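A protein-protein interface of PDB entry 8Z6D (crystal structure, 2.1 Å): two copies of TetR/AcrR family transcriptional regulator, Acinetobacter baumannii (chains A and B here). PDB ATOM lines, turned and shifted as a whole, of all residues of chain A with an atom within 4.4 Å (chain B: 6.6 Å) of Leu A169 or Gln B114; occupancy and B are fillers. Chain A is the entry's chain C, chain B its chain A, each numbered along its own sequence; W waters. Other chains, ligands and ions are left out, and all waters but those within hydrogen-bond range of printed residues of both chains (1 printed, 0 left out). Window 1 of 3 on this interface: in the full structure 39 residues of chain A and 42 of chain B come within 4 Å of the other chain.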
ATOM      1  N   PHE A 108      13.139 -19.642   2.635  1.00  0.00           N
ATOM      2  CA  PHE A 108      11.964 -20.438   2.282  1.00  0.00           C
ATOM      3  C   PHE A 108      11.492 -20.175   0.856  1.00  0.00           C
ATOM      4  O   PHE A 108      11.273 -19.022   0.454  1.00  0.00           O
ATOM      5  CB  PHE A 108      10.802 -20.169   3.231  1.00  0.00           C
ATOM      6  CG  PHE A 108       9.528 -20.874   2.829  1.00  0.00           C
ATOM      7  CD1 PHE A 108       9.434 -22.257   2.905  1.00  0.00           C
ATOM      8  CD2 PHE A 108       8.431 -20.158   2.360  1.00  0.00           C
ATOM      9  CE1 PHE A 108       8.271 -22.909   2.539  1.00  0.00           C
ATOM     10  CE2 PHE A 108       7.257 -20.805   1.999  1.00  0.00           C
ATOM     11  CZ  PHE A 108       7.172 -22.178   2.095  1.00  0.00           C
ATOM     12  N   GLN A 114       7.202 -30.880  -3.689  1.00  0.00           N
ATOM     13  CA  GLN A 114       6.192 -30.313  -4.576  1.00  0.00           C
ATOM     14  C   GLN A 114       6.843 -29.724  -5.827  1.00  0.00           C
ATOM     15  O   GLN A 114       6.439 -30.035  -6.950  1.00  0.00           O
ATOM     16  CB  GLN A 114       5.367 -29.253  -3.829  1.00  0.00           C
ATOM     17  CG  GLN A 114       4.489 -29.788  -2.662  1.00  0.00           C
ATOM     18  CD  GLN A 114       3.857 -28.667  -1.841  1.00  0.00           C
ATOM     19  OE1 GLN A 114       3.849 -27.499  -2.262  1.00  0.00           O
ATOM     20  NE2 GLN A 114       3.302 -29.020  -0.673  1.00  0.00           N
ATOM     21  N   TYR A 118       6.121 -30.717  -9.840  1.00  0.00           N
ATOM     22  CA  TYR A 118       5.600 -29.702 -10.757  1.00  0.00           C
ATOM     23  C   TYR A 118       6.560 -29.397 -11.898  1.00  0.00           C
ATOM     24  O   TYR A 118       6.119 -28.900 -12.944  1.00  0.00           O
ATOM     25  CB  TYR A 118       5.279 -28.420  -9.992  1.00  0.00           C
ATOM     26  CG  TYR A 118       3.853 -28.352  -9.494  1.00  0.00           C
ATOM     27  CD1 TYR A 118       2.791 -28.612 -10.345  1.00  0.00           C
ATOM     28  CD2 TYR A 118       3.572 -28.028  -8.176  1.00  0.00           C
ATOM     29  CE1 TYR A 118       1.495 -28.560  -9.905  1.00  0.00           C
ATOM     30  CE2 TYR A 118       2.266 -27.966  -7.723  1.00  0.00           C
ATOM     31  CZ  TYR A 118       1.242 -28.232  -8.592  1.00  0.00           C
ATOM     32  OH  TYR A 118      -0.045 -28.162  -8.147  1.00  0.00           O
ATOM     33  N   GLU A 165       0.110 -29.330   3.556  1.00  0.00           N
ATOM     34  CA  GLU A 165       0.725 -29.315   2.232  1.00  0.00           C
ATOM     35  C   GLU A 165       0.472 -27.993   1.525  1.00  0.00           C
ATOM     36  O   GLU A 165       1.398 -27.390   0.961  1.00  0.00           O
ATOM     37  CB  GLU A 165       0.204 -30.498   1.413  1.00  0.00           C
ATOM     38  CG  GLU A 165       0.876 -31.810   1.822  1.00  0.00           C
ATOM     39  CD  GLU A 165       2.397 -31.760   1.623  1.00  0.00           C
ATOM     40  OE1 GLU A 165       2.854 -31.841   0.454  1.00  0.00           O
ATOM     41  OE2 GLU A 165       3.137 -31.615   2.625  1.00  0.00           O
ATOM     42  N   GLY A 166      -0.762 -27.496   1.591  1.00  0.00           N
ATOM     43  CA  GLY A 166      -1.075 -26.248   0.933  1.00  0.00           C
ATOM     44  C   GLY A 166      -0.381 -25.053   1.554  1.00  0.00           C
ATOM     45  O   GLY A 166      -0.095 -24.080   0.861  1.00  0.00           O
ATOM     46  N   MET A 167      -0.132 -25.086   2.864  1.00  0.00           N
ATOM     47  CA  MET A 167       0.594 -23.984   3.482  1.00  0.00           C
ATOM     48  C   MET A 167       2.065 -23.946   3.097  1.00  0.00           C
ATOM     49  O   MET A 167       2.746 -22.962   3.404  1.00  0.00           O
ATOM     50  CB  MET A 167       0.479 -24.063   4.991  1.00  0.00           C
ATOM     51  CG  MET A 167      -0.943 -23.858   5.494  1.00  0.00           C
ATOM     52  SD  MET A 167      -1.032 -24.176   7.261  1.00  0.00           S
ATOM     53  CE  MET A 167       0.735 -24.424   7.598  1.00  0.00           C
ATOM     54  N   LEU A 168       2.570 -24.975   2.433  1.00  0.00           N
ATOM     55  CA  LEU A 168       3.952 -24.974   2.000  1.00  0.00           C
ATOM     56  C   LEU A 168       4.120 -24.408   0.595  1.00  0.00           C
ATOM     57  O   LEU A 168       5.238 -24.402   0.081  1.00  0.00           O
ATOM     58  CB  LEU A 168       4.522 -26.397   2.089  1.00  0.00           C
ATOM     59  CG  LEU A 168       4.655 -26.962   3.513  1.00  0.00           C
ATOM     60  CD1 LEU A 168       4.846 -28.484   3.517  1.00  0.00           C
ATOM     61  CD2 LEU A 168       5.793 -26.301   4.228  1.00  0.00           C
ATOM     62  N   LEU A 169       3.045 -23.925  -0.036  1.00  0.00           N
ATOM     63  CA  LEU A 169       3.185 -23.322  -1.355  1.00  0.00           C
ATOM     64  C   LEU A 169       4.015 -22.051  -1.255  1.00  0.00           C
ATOM     65  O   LEU A 169       3.953 -21.350  -0.242  1.00  0.00           O
ATOM     66  CB  LEU A 169       1.826 -22.985  -1.945  1.00  0.00           C
ATOM     67  CG  LEU A 169       1.014 -24.237  -2.231  1.00  0.00           C
ATOM     68  CD1 LEU A 169      -0.420 -23.838  -2.543  1.00  0.00           C
ATOM     69  CD2 LEU A 169       1.657 -25.005  -3.353  1.00  0.00           C
ATOM     70  N   PRO A 170       4.768 -21.716  -2.305  1.00  0.00           N
ATOM     71  CA  PRO A 170       5.512 -20.444  -2.309  1.00  0.00           C
ATOM     72  C   PRO A 170       4.610 -19.265  -1.957  1.00  0.00           C
ATOM     73  O   PRO A 170       3.461 -19.182  -2.392  1.00  0.00           O
ATOM     74  CB  PRO A 170       6.052 -20.333  -3.745  1.00  0.00           C
ATOM     75  CG  PRO A 170       5.879 -21.676  -4.393  1.00  0.00           C
ATOM     76  CD  PRO A 170       4.913 -22.494  -3.551  1.00  0.00           C
ATOM     77  N   ALA A 171       5.153 -18.324  -1.184  1.00  0.00           N
ATOM     78  CA  ALA A 171       4.332 -17.221  -0.675  1.00  0.00           C
ATOM     79  C   ALA A 171       3.754 -16.357  -1.798  1.00  0.00           C
ATOM     80  O   ALA A 171       2.626 -15.861  -1.691  1.00  0.00           O
ATOM     81  CB  ALA A 171       5.149 -16.363   0.289  1.00  0.00           C
ATOM     82  N   ILE A 173       2.424 -17.008  -4.528  1.00  0.00           N
ATOM     83  CA  ILE A 173       1.215 -17.463  -5.205  1.00  0.00           C
ATOM     84  C   ILE A 173      -0.005 -16.675  -4.721  1.00  0.00           C
ATOM     85  O   ILE A 173      -0.973 -16.491  -5.467  1.00  0.00           O
ATOM     86  CB  ILE A 173       1.037 -18.990  -5.027  1.00  0.00           C
ATOM     87  CG1 ILE A 173       0.026 -19.530  -6.043  1.00  0.00           C
ATOM     88  CG2 ILE A 173       0.626 -19.351  -3.601  1.00  0.00           C
ATOM     89  CD1 ILE A 173      -0.232 -21.003  -5.882  1.00  0.00           C
ATOM     90  N   GLY B 110      -2.326 -31.491 -11.450  1.00  0.00           N
ATOM     91  CA  GLY B 110      -2.059 -30.445 -10.488  1.00  0.00           C
ATOM     92  C   GLY B 110      -2.665 -29.109 -10.876  1.00  0.00           C
ATOM     93  O   GLY B 110      -3.402 -28.980 -11.852  1.00  0.00           O
ATOM     94  N   CYS B 111      -2.322 -28.091 -10.088  1.00  0.00           N
ATOM     95  CA  CYS B 111      -2.779 -26.725 -10.315  1.00  0.00           C
ATOM     96  C   CYS B 111      -1.766 -25.969 -11.176  1.00  0.00           C
ATOM     97  O   CYS B 111      -0.585 -25.885 -10.823  1.00  0.00           O
ATOM     98  CB  CYS B 111      -2.980 -26.014  -8.979  1.00  0.00           C
ATOM     99  SG  CYS B 111      -3.359 -24.275  -9.119  1.00  0.00           S
ATOM    100  N   LEU B 112      -2.229 -25.412 -12.299  1.00  0.00           N
ATOM    101  CA  LEU B 112      -1.336 -24.699 -13.210  1.00  0.00           C
ATOM    102  C   LEU B 112      -0.764 -23.420 -12.597  1.00  0.00           C
ATOM    103  O   LEU B 112       0.310 -22.963 -13.010  1.00  0.00           O
ATOM    104  CB  LEU B 112      -2.082 -24.373 -14.506  1.00  0.00           C
ATOM    105  CG  LEU B 112      -1.257 -24.060 -15.758  1.00  0.00           C
ATOM    106  CD1 LEU B 112      -0.435 -25.250 -16.257  1.00  0.00           C
ATOM    107  CD2 LEU B 112      -2.166 -23.593 -16.831  1.00  0.00           C
ATOM    108  N   PHE B 113      -1.447 -22.836 -11.614  1.00  0.00           N
ATOM    109  CA  PHE B 113      -0.932 -21.625 -10.995  1.00  0.00           C
ATOM    110  C   PHE B 113       0.165 -21.940 -10.000  1.00  0.00           C
ATOM    111  O   PHE B 113       1.155 -21.205  -9.924  1.00  0.00           O
ATOM    112  CB  PHE B 113      -2.072 -20.863 -10.324  1.00  0.00           C
ATOM    113  CG  PHE B 113      -3.180 -20.516 -11.262  1.00  0.00           C
ATOM    114  CD1 PHE B 113      -3.113 -19.377 -12.051  1.00  0.00           C
ATOM    115  CD2 PHE B 113      -4.275 -21.343 -11.394  1.00  0.00           C
ATOM    116  CE1 PHE B 113      -4.134 -19.061 -12.925  1.00  0.00           C
ATOM    117  CE2 PHE B 113      -5.290 -21.032 -12.267  1.00  0.00           C
ATOM    118  CZ  PHE B 113      -5.227 -19.891 -13.023  1.00  0.00           C
ATOM    119  N   GLN B 114      -0.015 -23.002  -9.205  1.00  0.00           N
ATOM    120  CA  GLN B 114       1.073 -23.495  -8.370  1.00  0.00           C
ATOM    121  C   GLN B 114       2.259 -23.913  -9.232  1.00  0.00           C
ATOM    122  O   GLN B 114       3.410 -23.667  -8.870  1.00  0.00           O
ATOM    123  CB  GLN B 114       0.602 -24.666  -7.501  1.00  0.00           C
ATOM    124  CG  GLN B 114      -0.709 -24.415  -6.722  1.00  0.00           C
ATOM    125  CD  GLN B 114      -1.247 -25.648  -6.003  1.00  0.00           C
ATOM    126  OE1 GLN B 114      -0.681 -26.739  -6.096  1.00  0.00           O
ATOM    127  NE2 GLN B 114      -2.374 -25.482  -5.300  1.00  0.00           N
ATOM    128  N   LYS B 115       1.998 -24.559 -10.369  1.00  0.00           N
ATOM    129  CA  LYS B 115       3.094 -24.954 -11.246  1.00  0.00           C
ATOM    130  C   LYS B 115       3.907 -23.738 -11.696  1.00  0.00           C
ATOM    131  O   LYS B 115       5.138 -23.786 -11.719  1.00  0.00           O
ATOM    132  CB  LYS B 115       2.571 -25.722 -12.471  1.00  0.00           C
ATOM    133  CG  LYS B 115       3.697 -26.380 -13.266  1.00  0.00           C
ATOM    134  CD  LYS B 115       3.302 -26.816 -14.673  1.00  0.00           C
ATOM    135  CE  LYS B 115       2.406 -28.050 -14.680  1.00  0.00           C
ATOM    136  NZ  LYS B 115       3.171 -29.283 -14.292  1.00  0.00           N
ATOM    137  N   ALA B 116       3.236 -22.644 -12.068  1.00  0.00           N
ATOM    138  CA  ALA B 116       3.969 -21.487 -12.571  1.00  0.00           C
ATOM    139  C   ALA B 116       4.865 -20.890 -11.492  1.00  0.00           C
ATOM    140  O   ALA B 116       5.993 -20.474 -11.781  1.00  0.00           O
ATOM    141  CB  ALA B 116       2.994 -20.442 -13.129  1.00  0.00           C
ATOM    142  N   VAL B 117       4.413 -20.874 -10.235  1.00  0.00           N
ATOM    143  CA  VAL B 117       5.263 -20.281  -9.199  1.00  0.00           C
ATOM    144  C   VAL B 117       6.432 -21.213  -8.872  1.00  0.00           C
ATOM    145  O   VAL B 117       7.547 -20.747  -8.611  1.00  0.00           O
ATOM    146  CB  VAL B 117       4.468 -19.871  -7.927  1.00  0.00           C
ATOM    147  CG1 VAL B 117       3.496 -18.698  -8.200  1.00  0.00           C
ATOM    148  CG2 VAL B 117       3.690 -21.029  -7.338  1.00  0.00           C
ATOM    149  N   TYR B 118       6.216 -22.539  -8.899  1.00  0.00           N
ATOM    150  CA  TYR B 118       7.319 -23.452  -8.595  1.00  0.00           C
ATOM    151  C   TYR B 118       8.375 -23.437  -9.691  1.00  0.00           C
ATOM    152  O   TYR B 118       9.562 -23.588  -9.400  1.00  0.00           O
ATOM    153  CB  TYR B 118       6.813 -24.874  -8.365  1.00  0.00           C
ATOM    154  CG  TYR B 118       6.474 -25.162  -6.907  1.00  0.00           C
ATOM    155  CD1 TYR B 118       7.428 -24.999  -5.902  1.00  0.00           C
ATOM    156  CD2 TYR B 118       5.190 -25.562  -6.532  1.00  0.00           C
ATOM    157  CE1 TYR B 118       7.115 -25.250  -4.553  1.00  0.00           C
ATOM    158  CE2 TYR B 118       4.860 -25.812  -5.191  1.00  0.00           C
ATOM    159  CZ  TYR B 118       5.834 -25.663  -4.214  1.00  0.00           C
ATOM    160  OH  TYR B 118       5.513 -25.907  -2.904  1.00  0.00           O
ATOM    161  N   GLU B 119       7.966 -23.228 -10.941  1.00  0.00           N
ATOM    162  CA  GLU B 119       8.857 -23.080 -12.082  1.00  0.00           C
ATOM    163  C   GLU B 119       9.390 -21.667 -12.243  1.00  0.00           C
ATOM    164  O   GLU B 119      10.178 -21.414 -13.159  1.00  0.00           O
ATOM    165  CB  GLU B 119       8.125 -23.516 -13.353  1.00  0.00           C
ATOM    166  CG  GLU B 119       7.842 -24.991 -13.360  1.00  0.00           C
ATOM    167  CD  GLU B 119       7.546 -25.498 -14.729  1.00  0.00           C
ATOM    168  OE1 GLU B 119       8.501 -25.764 -15.497  1.00  0.00           O
ATOM    169  OE2 GLU B 119       6.349 -25.633 -15.040  1.00  0.00           O
ATOM    170  N   ILE B 130      -1.876 -14.822 -11.507  1.00  0.00           N
ATOM    171  CA  ILE B 130      -1.859 -15.887 -10.504  1.00  0.00           C
ATOM    172  C   ILE B 130      -2.441 -15.382  -9.184  1.00  0.00           C
ATOM    173  O   ILE B 130      -3.362 -15.979  -8.617  1.00  0.00           O
ATOM    174  CB  ILE B 130      -0.421 -16.422 -10.333  1.00  0.00           C
ATOM    175  CG1 ILE B 130       0.029 -17.163 -11.585  1.00  0.00           C
ATOM    176  CG2 ILE B 130      -0.286 -17.320  -9.109  1.00  0.00           C
ATOM    177  CD1 ILE B 130       1.505 -17.529 -11.558  1.00  0.00           C
ATOM    178  N   LYS B 134      -5.932 -16.566  -7.245  1.00  0.00           N
ATOM    179  CA  LYS B 134      -5.967 -17.179  -5.922  1.00  0.00           C
ATOM    180  C   LYS B 134      -6.591 -16.235  -4.887  1.00  0.00           C
ATOM    181  O   LYS B 134      -7.217 -16.697  -3.926  1.00  0.00           O
ATOM    182  CB  LYS B 134      -4.560 -17.625  -5.504  1.00  0.00           C
ATOM    183  CG  LYS B 134      -3.986 -18.817  -6.299  1.00  0.00           C
ATOM    184  CD  LYS B 134      -4.961 -20.010  -6.370  1.00  0.00           C
ATOM    185  CE  LYS B 134      -4.338 -21.171  -7.135  1.00  0.00           C
ATOM    186  NZ  LYS B 134      -5.182 -22.416  -7.087  1.00  0.00           N
ATOM    187  N   TYR B 161      -9.367 -23.231   2.600  1.00  0.00           N
ATOM    188  CA  TYR B 161      -8.654 -22.778   1.409  1.00  0.00           C
ATOM    189  C   TYR B 161      -7.344 -23.531   1.227  1.00  0.00           C
ATOM    190  O   TYR B 161      -7.068 -24.071   0.152  1.00  0.00           O
ATOM    191  CB  TYR B 161      -8.370 -21.280   1.508  1.00  0.00           C
ATOM    192  CG  TYR B 161      -7.416 -20.766   0.454  1.00  0.00           C
ATOM    193  CD1 TYR B 161      -7.886 -20.340  -0.781  1.00  0.00           C
ATOM    194  CD2 TYR B 161      -6.035 -20.684   0.694  1.00  0.00           C
ATOM    195  CE1 TYR B 161      -7.017 -19.861  -1.770  1.00  0.00           C
ATOM    196  CE2 TYR B 161      -5.152 -20.203  -0.289  1.00  0.00           C
ATOM    197  CZ  TYR B 161      -5.663 -19.787  -1.523  1.00  0.00           C
ATOM    198  OH  TYR B 161      -4.826 -19.300  -2.518  1.00  0.00           O
ATOM    199  N   SER B 162      -6.489 -23.522   2.251  1.00  0.00           N
ATOM    200  CA  SER B 162      -5.210 -24.217   2.122  1.00  0.00           C
ATOM    201  C   SER B 162      -5.394 -25.717   1.924  1.00  0.00           C
ATOM    202  O   SER B 162      -4.631 -26.326   1.175  1.00  0.00           O
ATOM    203  CB  SER B 162      -4.332 -23.936   3.328  1.00  0.00           C
ATOM    204  OG  SER B 162      -3.958 -22.583   3.303  1.00  0.00           O
ATOM    205  N   LEU B 164      -7.894 -27.219   0.276  1.00  0.00           N
ATOM    206  CA  LEU B 164      -8.211 -27.331  -1.143  1.00  0.00           C
ATOM    207  C   LEU B 164      -6.986 -27.088  -2.017  1.00  0.00           C
ATOM    208  O   LEU B 164      -6.784 -27.780  -3.020  1.00  0.00           O
ATOM    209  CB  LEU B 164      -9.320 -26.345  -1.509  1.00  0.00           C
ATOM    210  CG  LEU B 164     -10.670 -26.580  -0.852  1.00  0.00           C
ATOM    211  CD1 LEU B 164     -11.640 -25.440  -1.205  1.00  0.00           C
ATOM    212  CD2 LEU B 164     -11.202 -27.937  -1.300  1.00  0.00           C
ATOM    213  N   GLU B 165      -6.166 -26.098  -1.669  1.00  0.00           N
ATOM    214  CA  GLU B 165      -4.926 -25.886  -2.408  1.00  0.00           C
ATOM    215  C   GLU B 165      -4.011 -27.110  -2.325  1.00  0.00           C
ATOM    216  O   GLU B 165      -3.381 -27.497  -3.323  1.00  0.00           O
ATOM    217  CB  GLU B 165      -4.218 -24.630  -1.890  1.00  0.00           C
ATOM    218  CG  GLU B 165      -4.819 -23.315  -2.429  1.00  0.00           C
ATOM    219  CD  GLU B 165      -4.701 -23.162  -3.936  1.00  0.00           C
ATOM    220  OE1 GLU B 165      -3.568 -22.936  -4.421  1.00  0.00           O
ATOM    221  OE2 GLU B 165      -5.747 -23.249  -4.635  1.00  0.00           O
ATOM    222  N   GLY B 166      -3.922 -27.734  -1.146  1.00  0.00           N
ATOM    223  CA  GLY B 166      -3.100 -28.932  -1.015  1.00  0.00           C
ATOM    224  C   GLY B 166      -3.691 -30.146  -1.718  1.00  0.00           C
ATOM    225  O   GLY B 166      -2.956 -31.045  -2.153  1.00  0.00           O
ATOM    226  N   MET B 167      -5.015 -30.189  -1.841  1.00  0.00           N
ATOM    227  CA  MET B 167      -5.686 -31.202  -2.631  1.00  0.00           C
ATOM    228  C   MET B 167      -5.512 -31.016  -4.128  1.00  0.00           C
ATOM    229  O   MET B 167      -5.896 -31.912  -4.878  1.00  0.00           O
ATOM    230  CB  MET B 167      -7.164 -31.236  -2.276  1.00  0.00           C
ATOM    231  CG  MET B 167      -7.436 -32.002  -1.005  1.00  0.00           C
ATOM    232  SD  MET B 167      -9.089 -31.702  -0.337  1.00  0.00           S
ATOM    233  CE  MET B 167      -8.971 -32.594   1.230  1.00  0.00           C
ATOM    234  N   LEU B 168      -4.948 -29.900  -4.585  1.00  0.00           N
ATOM    235  CA  LEU B 168      -4.706 -29.711  -6.007  1.00  0.00           C
ATOM    236  C   LEU B 168      -3.302 -30.125  -6.424  1.00  0.00           C
ATOM    237  O   LEU B 168      -2.932 -29.923  -7.581  1.00  0.00           O
ATOM    238  CB  LEU B 168      -4.977 -28.261  -6.404  1.00  0.00           C
ATOM    239  CG  LEU B 168      -6.451 -27.829  -6.393  1.00  0.00           C
ATOM    240  CD1 LEU B 168      -6.528 -26.333  -6.675  1.00  0.00           C
ATOM    241  CD2 LEU B 168      -7.270 -28.605  -7.423  1.00  0.00           C
ATOM    242  N   LEU B 169      -2.522 -30.696  -5.519  1.00  0.00           N
ATOM    243  CA  LEU B 169      -1.185 -31.162  -5.858  1.00  0.00           C
ATOM    244  C   LEU B 169      -1.277 -32.348  -6.817  1.00  0.00           C
ATOM    245  O   LEU B 169      -2.245 -33.102  -6.785  1.00  0.00           O
ATOM    246  CB  LEU B 169      -0.432 -31.554  -4.590  1.00  0.00           C
ATOM    247  CG  LEU B 169      -0.061 -30.373  -3.684  1.00  0.00           C
ATOM    248  CD1 LEU B 169       0.384 -30.819  -2.268  1.00  0.00           C
ATOM    249  CD2 LEU B 169       0.985 -29.503  -4.349  1.00  0.00           C
ATOM    250  N   PRO B 170      -0.292 -32.522  -7.696  1.00  0.00           N
ATOM    251  CA  PRO B 170      -0.307 -33.685  -8.592  1.00  0.00           C
ATOM    252  C   PRO B 170      -0.398 -34.969  -7.785  1.00  0.00           C
ATOM    253  O   PRO B 170       0.232 -35.096  -6.736  1.00  0.00           O
ATOM    254  CB  PRO B 170       1.026 -33.581  -9.331  1.00  0.00           C
ATOM    255  CG  PRO B 170       1.411 -32.122  -9.219  1.00  0.00           C
ATOM    256  CD  PRO B 170       0.895 -31.670  -7.890  1.00  0.00           C
HETATM  257  O   HOH W   1      -2.284 -22.300   0.812  1.00  0.00           O
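The side-chain amide nitrogen (NE2) of Gln B114 is in hydrogen-bond range of the side-chain carboxylate (OE1) of Glu B165, at 2.9 Å. The backbone carbonyl oxygen of Leu B168 lies within hydrogen-bond range of the backbone NH of Cys B111, at 3.2 Å. NE2 of Gln A114 is in hydrogen-bond range of O of Glu A165, at 3.0 Å. SG of Cys B111 sits close to N of Gln B114, at 3.6 Å. SG of Cys B111 sits close to N of Phe B113 (3.5 Å). The side-chain amino group of Lys B134 sits at hydrogen-bond distance from the side-chain sulfur of Cys B111 (3.3 Å).
Water W1 lies within hydrogen-bond range of O of Gly A166 (2.8 Å) and OG of Ser B162 (3.0 Å).
Gln A114 touches Leu B169, and with the chains exchanged Leu A169 touches Gln B114. Tyr A118 touches Leu B168, and with the chains exchanged Leu A168 touches Tyr B118. Tyr A118 touches Pro B170, and with the chains exchanged Pro A170 touches Tyr B118. Gly B166 touches its own counterpart, Gly A166. 8 positions are printed for both chains.
The side-chain hydroxyl of Tyr B118 sits close to the side-chain amide oxygen of Gln A114 (2.4 Å). The side-chain hydroxyl (OH) of Tyr A118 lies within hydrogen-bond range of the backbone carbonyl oxygen (O) of Leu B168. OH of Tyr A118 lies within hydrogen-bond range of N of Cys B111 (3.0 Å). The side-chain amino group of Lys B115 sits at hydrogen-bond distance from the backbone carbonyl oxygen of Tyr A118 (3.3 Å). The backbone carbonyl oxygen of Leu A168 sits at hydrogen-bond distance from the side-chain hydroxyl of Tyr B118 (3.4 Å). The side-chain amide oxygen of Gln B114 is in hydrogen-bond range of the side-chain hydroxyl of Tyr A118 (2.6 Å).
Printed residues of chain A within 4 Å of Gln B114: Tyr A118 (2.6 Å), Leu A169 (3.8 Å) and Ile A173 (3.5 Å). Of the printed residues of chain B, Gly A166 touches Ser B162 (3.6 Å) and Gly B166 (3.8 Å). Of the printed residues of chain B, Pro A170 touches Val B117 and Tyr B118. Of the printed residues of chain A, Lys B134 touches Ile A173 (3.8 Å). Printed residues of chain A within 4 Å of Val B117: Pro A170 and Ile A173. Of the printed residues of chain A, Tyr B118 touches Gln A114, Tyr A118, Leu A168, Leu A169 and Pro A170. Ala B116 touches none of the printed residues of chain A. Met B167 touches none of the printed residues of chain A. The nearest residue of chain B that does not touch Leu A169 is Leu B169 (4.7 Å). The nearest printed residue of chain A that does not touch Gln B114 is Pro A170 (5.5 Å).
Among the printed residues, pairs that only touch across the chains: Pro A170 with Tyr B118 (3.4 Å), Tyr A118 with Tyr B118 (3.4 Å), Tyr A118 with Pro B170 (3.5 Å), Ile A173 with Gln B114 (3.5 Å), Gly A166 with Ser B162 (3.6 Å), Glu A165 with Leu B169 (3.7 Å), Pro A170 with Val B117 (3.7 Å), Leu A169 with Gln B114 (3.8 Å), Ile A173 with Lys B134 (3.8 Å), Leu A169 with Glu B165 (3.8 Å), Leu A169 with Tyr B118 (3.8 Å), Gln A114 with Leu B169 (3.8 Å), Gly A166 with Gly B166 (3.8 Å), Ile A173 with Ile B130 (3.8 Å), Tyr A118 with Gly B110 (3.8 Å), Tyr A118 with Glu B119 (3.9 Å), Tyr A118 with Leu B169 (3.9 Å), Met A167 with Ser B162 (3.9 Å) and Ile A173 with Val B117 (3.96 Å).
Hydrophobic or aromatic side chains of chain A that line the printed part of chain B: Tyr A118, Met A167, Leu A169, Pro A170 and Ile A173. Among the printed residues, 25 pairs touch across the chains. Among the printed residues, no Asp or Glu carboxylate lies within 4 Å of a Lys or Arg side-chain nitrogen of the other chain.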
